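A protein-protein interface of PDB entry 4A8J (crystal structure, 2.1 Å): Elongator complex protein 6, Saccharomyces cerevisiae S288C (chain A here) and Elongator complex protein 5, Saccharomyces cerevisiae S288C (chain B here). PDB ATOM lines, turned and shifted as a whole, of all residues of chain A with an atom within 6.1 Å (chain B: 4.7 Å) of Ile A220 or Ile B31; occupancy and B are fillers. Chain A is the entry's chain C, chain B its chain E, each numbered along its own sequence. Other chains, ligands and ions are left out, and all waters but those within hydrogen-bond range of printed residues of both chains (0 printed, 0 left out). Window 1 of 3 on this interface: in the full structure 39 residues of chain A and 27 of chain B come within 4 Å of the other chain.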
ATOM      1  N   TYR A 215     -24.038  15.671 -15.659  1.00  0.00           N
ATOM      2  CA  TYR A 215     -24.237  17.108 -15.503  1.00  0.00           C
ATOM      3  C   TYR A 215     -23.652  17.805 -16.717  1.00  0.00           C
ATOM      4  O   TYR A 215     -24.271  18.707 -17.289  1.00  0.00           O
ATOM      5  CB  TYR A 215     -23.576  17.606 -14.206  1.00  0.00           C
ATOM      6  CG  TYR A 215     -24.222  17.024 -12.964  1.00  0.00           C
ATOM      7  CD1 TYR A 215     -23.938  15.734 -12.556  1.00  0.00           C
ATOM      8  CD2 TYR A 215     -25.153  17.755 -12.231  1.00  0.00           C
ATOM      9  CE1 TYR A 215     -24.542  15.184 -11.424  1.00  0.00           C
ATOM     10  CE2 TYR A 215     -25.774  17.216 -11.107  1.00  0.00           C
ATOM     11  CZ  TYR A 215     -25.456  15.930 -10.705  1.00  0.00           C
ATOM     12  OH  TYR A 215     -26.058  15.389  -9.589  1.00  0.00           O
ATOM     13  N   LYS A 216     -22.472  17.361 -17.151  1.00  0.00           N
ATOM     14  CA  LYS A 216     -21.912  17.975 -18.362  1.00  0.00           C
ATOM     15  C   LYS A 216     -22.752  17.754 -19.608  1.00  0.00           C
ATOM     16  O   LYS A 216     -22.988  18.674 -20.407  1.00  0.00           O
ATOM     17  CB  LYS A 216     -20.516  17.443 -18.627  1.00  0.00           C
ATOM     18  CG  LYS A 216     -19.584  17.572 -17.461  1.00  0.00           C
ATOM     19  CD  LYS A 216     -19.110  18.979 -17.264  1.00  0.00           C
ATOM     20  CE  LYS A 216     -18.013  18.957 -16.206  1.00  0.00           C
ATOM     21  NZ  LYS A 216     -17.069  17.828 -16.499  1.00  0.00           N
ATOM     22  N   SER A 217     -23.194  16.520 -19.819  1.00  0.00           N
ATOM     23  CA  SER A 217     -23.969  16.240 -21.027  1.00  0.00           C
ATOM     24  C   SER A 217     -25.335  16.957 -20.937  1.00  0.00           C
ATOM     25  O   SER A 217     -25.835  17.517 -21.926  1.00  0.00           O
ATOM     26  CB  SER A 217     -24.125  14.734 -21.253  1.00  0.00           C
ATOM     27  OG  SER A 217     -24.747  14.141 -20.120  1.00  0.00           O
ATOM     28  N   SER A 218     -25.943  16.958 -19.752  1.00  0.00           N
ATOM     29  CA  SER A 218     -27.217  17.679 -19.614  1.00  0.00           C
ATOM     30  C   SER A 218     -27.032  19.160 -19.980  1.00  0.00           C
ATOM     31  O   SER A 218     -27.838  19.749 -20.703  1.00  0.00           O
ATOM     32  CB  SER A 218     -27.766  17.531 -18.192  1.00  0.00           C
ATOM     33  OG  SER A 218     -28.257  16.220 -18.001  1.00  0.00           O
ATOM     34  N   PHE A 219     -25.954  19.757 -19.483  1.00  0.00           N
ATOM     35  CA  PHE A 219     -25.689  21.149 -19.799  1.00  0.00           C
ATOM     36  C   PHE A 219     -25.564  21.355 -21.308  1.00  0.00           C
ATOM     37  O   PHE A 219     -26.173  22.269 -21.898  1.00  0.00           O
ATOM     38  CB  PHE A 219     -24.398  21.589 -19.146  1.00  0.00           C
ATOM     39  CG  PHE A 219     -24.079  23.027 -19.394  1.00  0.00           C
ATOM     40  CD1 PHE A 219     -24.593  24.015 -18.563  1.00  0.00           C
ATOM     41  CD2 PHE A 219     -23.289  23.400 -20.477  1.00  0.00           C
ATOM     42  CE1 PHE A 219     -24.310  25.359 -18.802  1.00  0.00           C
ATOM     43  CE2 PHE A 219     -22.991  24.733 -20.710  1.00  0.00           C
ATOM     44  CZ  PHE A 219     -23.504  25.719 -19.875  1.00  0.00           C
ATOM     45  N   ILE A 220     -24.756  20.496 -21.928  1.00  0.00           N
ATOM     46  CA  ILE A 220     -24.532  20.554 -23.361  1.00  0.00           C
ATOM     47  C   ILE A 220     -25.834  20.513 -24.171  1.00  0.00           C
ATOM     48  O   ILE A 220     -25.987  21.246 -25.165  1.00  0.00           O
ATOM     49  CB  ILE A 220     -23.532  19.444 -23.801  1.00  0.00           C
ATOM     50  CG1 ILE A 220     -22.128  19.816 -23.326  1.00  0.00           C
ATOM     51  CG2 ILE A 220     -23.554  19.252 -25.309  1.00  0.00           C
ATOM     52  CD1 ILE A 220     -21.170  18.621 -23.275  1.00  0.00           C
ATOM     53  N   LYS A 221     -26.775  19.670 -23.759  1.00  0.00           N
ATOM     54  CA  LYS A 221     -28.048  19.583 -24.485  1.00  0.00           C
ATOM     55  C   LYS A 221     -29.046  20.713 -24.157  1.00  0.00           C
ATOM     56  O   LYS A 221     -30.029  20.905 -24.856  1.00  0.00           O
ATOM     57  CB  LYS A 221     -28.694  18.212 -24.221  1.00  0.00           C
ATOM     58  CG  LYS A 221     -27.927  17.032 -24.830  1.00  0.00           C
ATOM     59  CD  LYS A 221     -28.766  15.751 -24.851  1.00  0.00           C
ATOM     60  CE  LYS A 221     -28.847  15.141 -23.484  1.00  0.00           C
ATOM     61  NZ  LYS A 221     -27.539  15.313 -22.806  1.00  0.00           N
ATOM     62  N   SER A 222     -28.817  21.453 -23.081  1.00  0.00           N
ATOM     63  CA  SER A 222     -29.822  22.424 -22.643  1.00  0.00           C
ATOM     64  C   SER A 222     -29.654  23.762 -23.362  1.00  0.00           C
ATOM     65  O   SER A 222     -28.536  24.135 -23.745  1.00  0.00           O
ATOM     66  CB  SER A 222     -29.711  22.658 -21.136  1.00  0.00           C
ATOM     67  OG  SER A 222     -28.518  23.370 -20.859  1.00  0.00           O
ATOM     68  N   MET A 223     -30.750  24.495 -23.534  1.00  0.00           N
ATOM     69  CA  MET A 223     -30.618  25.855 -24.054  1.00  0.00           C
ATOM     70  C   MET A 223     -30.575  26.900 -22.947  1.00  0.00           C
ATOM     71  O   MET A 223     -30.341  28.078 -23.214  1.00  0.00           O
ATOM     72  CB  MET A 223     -31.670  26.191 -25.125  1.00  0.00           C
ATOM     73  CG  MET A 223     -33.032  25.546 -24.969  1.00  0.00           C
ATOM     74  SD  MET A 223     -34.165  26.294 -23.521  1.00  0.00           S
ATOM     75  CE  MET A 223     -33.614  28.078 -23.530  1.00  0.00           C
ATOM     76  N   GLY A 248     -27.250  27.664 -22.010  1.00  0.00           N
ATOM     77  CA  GLY A 248     -26.799  26.279 -21.991  1.00  0.00           C
ATOM     78  C   GLY A 248     -25.925  26.051 -23.221  1.00  0.00           C
ATOM     79  O   GLY A 248     -25.538  27.008 -23.888  1.00  0.00           O
ATOM     80  N   GLY A 249     -25.617  24.796 -23.545  1.00  0.00           N
ATOM     81  CA  GLY A 249     -24.696  24.524 -24.633  1.00  0.00           C
ATOM     82  C   GLY A 249     -25.374  24.406 -25.989  1.00  0.00           C
ATOM     83  O   GLY A 249     -24.707  24.275 -27.003  1.00  0.00           O
ATOM     84  N   ALA A 250     -26.707  24.454 -26.009  1.00  0.00           N
ATOM     85  CA  ALA A 250     -27.453  24.239 -27.244  1.00  0.00           C
ATOM     86  C   ALA A 250     -28.254  25.479 -27.627  1.00  0.00           C
ATOM     87  O   ALA A 250     -28.610  26.284 -26.758  1.00  0.00           O
ATOM     88  CB  ALA A 250     -28.372  23.039 -27.106  1.00  0.00           C
ATOM     89  N   SER B  30     -16.105  21.990 -25.236  1.00  0.00           N
ATOM     90  CA  SER B  30     -16.293  21.856 -23.799  1.00  0.00           C
ATOM     91  C   SER B  30     -17.546  22.616 -23.385  1.00  0.00           C
ATOM     92  O   SER B  30     -18.134  23.352 -24.193  1.00  0.00           O
ATOM     93  CB  SER B  30     -15.087  22.422 -23.062  1.00  0.00           C
ATOM     94  OG  SER B  30     -15.036  23.832 -23.207  1.00  0.00           O
ATOM     95  N   ILE B  31     -17.966  22.471 -22.127  1.00  0.00           N
ATOM     96  CA  ILE B  31     -19.216  23.135 -21.744  1.00  0.00           C
ATOM     97  C   ILE B  31     -19.150  24.659 -21.867  1.00  0.00           C
ATOM     98  O   ILE B  31     -20.181  25.318 -22.060  1.00  0.00           O
ATOM     99  CB  ILE B  31     -19.726  22.703 -20.361  1.00  0.00           C
ATOM    100  CG1 ILE B  31     -18.703  23.035 -19.278  1.00  0.00           C
ATOM    101  CG2 ILE B  31     -20.023  21.202 -20.364  1.00  0.00           C
ATOM    102  CD1 ILE B  31     -19.266  22.818 -17.840  1.00  0.00           C
ATOM    103  N   ALA B  32     -17.949  25.223 -21.748  1.00  0.00           N
ATOM    104  CA  ALA B  32     -17.769  26.678 -21.850  1.00  0.00           C
ATOM    105  C   ALA B  32     -18.004  27.207 -23.274  1.00  0.00           C
ATOM    106  O   ALA B  32     -18.313  28.391 -23.478  1.00  0.00           O
ATOM    107  CB  ALA B  32     -16.385  27.082 -21.349  1.00  0.00           C
ATOM    108  N   GLN B  33     -17.847  26.336 -24.266  1.00  0.00           N
ATOM    109  CA  GLN B  33     -18.117  26.716 -25.653  1.00  0.00           C
ATOM    110  C   GLN B  33     -18.291  25.483 -26.496  1.00  0.00           C
ATOM    111  O   GLN B  33     -17.317  24.827 -26.849  1.00  0.00           O
ATOM    112  CB  GLN B  33     -16.989  27.580 -26.240  1.00  0.00           C
ATOM    113  CG  GLN B  33     -17.348  28.157 -27.629  1.00  0.00           C
ATOM    114  CD  GLN B  33     -18.256  29.406 -27.565  1.00  0.00           C
ATOM    115  OE1 GLN B  33     -18.049  30.287 -26.736  1.00  0.00           O
ATOM    116  NE2 GLN B  33     -19.246  29.487 -28.465  1.00  0.00           N
ATOM    117  N   THR B  34     -19.528  25.150 -26.817  1.00  0.00           N
ATOM    118  CA  THR B  34     -19.785  23.907 -27.524  1.00  0.00           C
ATOM    119  C   THR B  34     -19.501  24.096 -29.002  1.00  0.00           C
ATOM    120  O   THR B  34     -19.144  25.188 -29.408  1.00  0.00           O
ATOM    121  CB  THR B  34     -21.204  23.447 -27.330  1.00  0.00           C
ATOM    122  OG1 THR B  34     -22.099  24.481 -27.779  1.00  0.00           O
ATOM    123  CG2 THR B  34     -21.424  23.126 -25.825  1.00  0.00           C
ATOM    124  N   GLU B  61     -26.884  12.798 -29.457  1.00  0.00           N
ATOM    125  CA  GLU B  61     -27.419  13.693 -28.433  1.00  0.00           C
ATOM    126  C   GLU B  61     -28.140  14.931 -28.982  1.00  0.00           C
ATOM    127  O   GLU B  61     -28.348  15.897 -28.263  1.00  0.00           O
ATOM    128  CB  GLU B  61     -26.307  14.096 -27.461  1.00  0.00           C
ATOM    129  CG  GLU B  61     -25.246  14.943 -28.101  1.00  0.00           C
ATOM    130  CD  GLU B  61     -24.051  15.186 -27.196  1.00  0.00           C
ATOM    131  OE1 GLU B  61     -23.898  14.480 -26.169  1.00  0.00           O
ATOM    132  OE2 GLU B  61     -23.260  16.097 -27.520  1.00  0.00           O
ATOM    133  N   HIS B 136     -16.165  15.963 -26.955  1.00  0.00           N
ATOM    134  CA  HIS B 136     -16.248  16.860 -25.798  1.00  0.00           C
ATOM    135  C   HIS B 136     -15.085  16.566 -24.874  1.00  0.00           C
ATOM    136  O   HIS B 136     -15.017  15.474 -24.298  1.00  0.00           O
ATOM    137  CB  HIS B 136     -17.553  16.658 -25.031  1.00  0.00           C
ATOM    138  CG  HIS B 136     -18.787  16.769 -25.873  1.00  0.00           C
ATOM    139  ND1 HIS B 136     -19.006  17.824 -26.747  1.00  0.00           N
ATOM    140  CD2 HIS B 136     -19.884  15.987 -25.950  1.00  0.00           C
ATOM    141  CE1 HIS B 136     -20.172  17.661 -27.344  1.00  0.00           C
ATOM    142  NE2 HIS B 136     -20.734  16.557 -26.875  1.00  0.00           N
ATOM    143  N   ASP B 138     -14.443  17.420 -21.990  1.00  0.00           N
ATOM    144  CA  ASP B 138     -14.703  17.307 -20.547  1.00  0.00           C
ATOM    145  C   ASP B 138     -15.710  16.216 -20.167  1.00  0.00           C
ATOM    146  O   ASP B 138     -16.196  16.175 -19.041  1.00  0.00           O
ATOM    147  CB  ASP B 138     -15.111  18.668 -19.947  1.00  0.00           C
ATOM    148  CG  ASP B 138     -16.223  19.375 -20.750  1.00  0.00           C
ATOM    149  OD1 ASP B 138     -16.774  18.778 -21.699  1.00  0.00           O
ATOM    150  OD2 ASP B 138     -16.553  20.538 -20.418  1.00  0.00           O
ATOM    151  N   ILE B 139     -16.032  15.347 -21.121  1.00  0.00           N
ATOM    152  CA  ILE B 139     -16.816  14.141 -20.859  1.00  0.00           C
ATOM    153  C   ILE B 139     -15.829  12.978 -20.744  1.00  0.00           C
ATOM    154  O   ILE B 139     -15.072  12.712 -21.681  1.00  0.00           O
ATOM    155  CB  ILE B 139     -17.788  13.846 -22.019  1.00  0.00           C
ATOM    156  CG1 ILE B 139     -18.844  14.960 -22.152  1.00  0.00           C
ATOM    157  CG2 ILE B 139     -18.414  12.458 -21.873  1.00  0.00           C
ATOM    158  CD1 ILE B 139     -19.847  15.014 -21.038  1.00  0.00           C
ATOM    159  N   LEU B 188     -16.336  26.487 -12.830  1.00  0.00           N
ATOM    160  CA  LEU B 188     -16.837  25.351 -13.609  1.00  0.00           C
ATOM    161  C   LEU B 188     -16.582  24.019 -12.866  1.00  0.00           C
ATOM    162  O   LEU B 188     -17.389  23.084 -12.949  1.00  0.00           O
ATOM    163  CB  LEU B 188     -16.224  25.325 -15.014  1.00  0.00           C
ATOM    164  CG  LEU B 188     -16.602  26.424 -16.011  1.00  0.00           C
ATOM    165  CD1 LEU B 188     -15.831  26.254 -17.336  1.00  0.00           C
ATOM    166  CD2 LEU B 188     -18.113  26.467 -16.260  1.00  0.00           C
ATOM    167  N   PHE B 191     -19.358  23.459 -10.652  1.00  0.00           N
ATOM    168  CA  PHE B 191     -20.607  23.646 -11.415  1.00  0.00           C
ATOM    169  C   PHE B 191     -21.395  24.912 -11.054  1.00  0.00           C
ATOM    170  O   PHE B 191     -22.632  24.956 -11.142  1.00  0.00           O
ATOM    171  CB  PHE B 191     -21.508  22.403 -11.384  1.00  0.00           C
ATOM    172  CG  PHE B 191     -22.116  22.080 -12.719  1.00  0.00           C
ATOM    173  CD1 PHE B 191     -21.401  21.367 -13.664  1.00  0.00           C
ATOM    174  CD2 PHE B 191     -23.395  22.523 -13.045  1.00  0.00           C
ATOM    175  CE1 PHE B 191     -21.945  21.086 -14.919  1.00  0.00           C
ATOM    176  CE2 PHE B 191     -23.945  22.246 -14.301  1.00  0.00           C
ATOM    177  CZ  PHE B 191     -23.222  21.517 -15.230  1.00  0.00           C
ATOM    178  N   ILE B 193     -21.890  27.677 -12.828  1.00  0.00           N
ATOM    179  CA  ILE B 193     -21.710  28.171 -14.186  1.00  0.00           C
ATOM    180  C   ILE B 193     -21.840  29.690 -14.236  1.00  0.00           C
ATOM    181  O   ILE B 193     -22.871  30.243 -13.859  1.00  0.00           O
ATOM    182  CB  ILE B 193     -22.765  27.578 -15.137  1.00  0.00           C
ATOM    183  CG1 ILE B 193     -22.863  26.061 -14.930  1.00  0.00           C
ATOM    184  CG2 ILE B 193     -22.438  27.927 -16.588  1.00  0.00           C
ATOM    185  CD1 ILE B 193     -21.569  25.324 -15.191  1.00  0.00           C
ATOM    186  N   ASN B 198     -20.255  30.528 -23.973  1.00  0.00           N
ATOM    187  CA  ASN B 198     -21.057  30.118 -25.115  1.00  0.00           C
ATOM    188  C   ASN B 198     -21.488  31.304 -25.994  1.00  0.00           C
ATOM    189  O   ASN B 198     -22.657  31.449 -26.346  1.00  0.00           O
ATOM    190  CB  ASN B 198     -22.237  29.276 -24.628  1.00  0.00           C
ATOM    191  CG  ASN B 198     -21.816  27.837 -24.301  1.00  0.00           C
ATOM    192  OD1 ASN B 198     -21.565  27.023 -25.210  1.00  0.00           O
ATOM    193  ND2 ASN B 198     -21.692  27.532 -22.999  1.00  0.00           N
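The side-chain hydroxyl (OG1) of Thr B34 is in hydrogen-bond range of the backbone carbonyl oxygen (O) of Gly A249.
O of Asp B138 sits at hydrogen-bond distance from NZ of Lys A216 (3.2 Å).
N of Thr B34 lies within hydrogen-bond range of OD1 of Asn B198.
The backbone carbonyl oxygen (O) of Phe A219 lies within hydrogen-bond range of the side-chain hydroxyl (OG) of Ser A222, 2.8 Å away.
The backbone carbonyl oxygen of Phe A219 lies within hydrogen-bond range of the backbone NH of Gly A249 (3.1 Å).
The backbone carbonyl oxygen (O) of Met A223 is in hydrogen-bond range of the backbone NH (N) of Gly A248 (3.3 Å).
The backbone carbonyl oxygen (O) of Ile A220 is in hydrogen-bond range of the backbone NH (N) of Ala A250 (3.4 Å).
N of Ile B31 sits at hydrogen-bond distance from OD2 of Asp B138, 2.9 Å away.
Among the printed residues, merely in contact across the chains: Tyr A215 with Phe B191 (3.6 Å), Lys A216 with Ile B31 (3.9 Å), Lys A216 with Ile B139 (3.5 Å), Ser A217 with Ile B139 (3.9 Å), Phe A219 with Ile B31 (3.2 Å), Phe A219 with Ile B193 (3.9 Å), Phe A219 with Asn B198 (3.8 Å), Ile A220 with Ile B31 (3.9 Å), Ile A220 with Glu B61 (3.9 Å), Ile A220 with His B136 (3.97 Å), Lys A221 with Glu B61 (3.4 Å) and Gly A248 with Asn B198 (3.8 Å).
Ile A220 touches three residues of chain B.
Of the printed residues of chain A, Asn B198 touches Phe A219 and Gly A248.
Of the printed residues of chain A, His B136 touches Ile A220 (3.97 Å).
Of the printed residues of chain A, Ile B139 touches Lys A216 (3.5 Å) and Ser A217 (3.9 Å).
Of the printed residues of chain A, Asp B138 touches Lys A216 (3.2 Å).
Ser A218 touches none of the printed residues of chain B.
The nearest residue of chain A that does not touch Ile B31 is Gly A249 (5.3 Å).
Printed residues of chain B that touch a printed residue of chain A: Ile B31, Thr B34, Glu B61, His B136, Asp B138, Ile B139, Phe B191, Ile B193 and Asn B198.
Hydrophobic or aromatic side chains of chain B that line the printed part of chain A: Ile B31, His B136, Ile B139, Phe B191 and Ile B193.
Of the 12 printed residues of chain A, 8 touch a printed residue of chain B.
Printed residues of chain A that touch a printed residue of chain B: Tyr A215, Lys A216, Ser A217, Phe A219, Ile A220, Lys A221, Gly A248 and Gly A249.
Hydrophobic or aromatic side chains of chain A that line the printed part of chain B: Tyr A215, Phe A219 and Ile A220.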
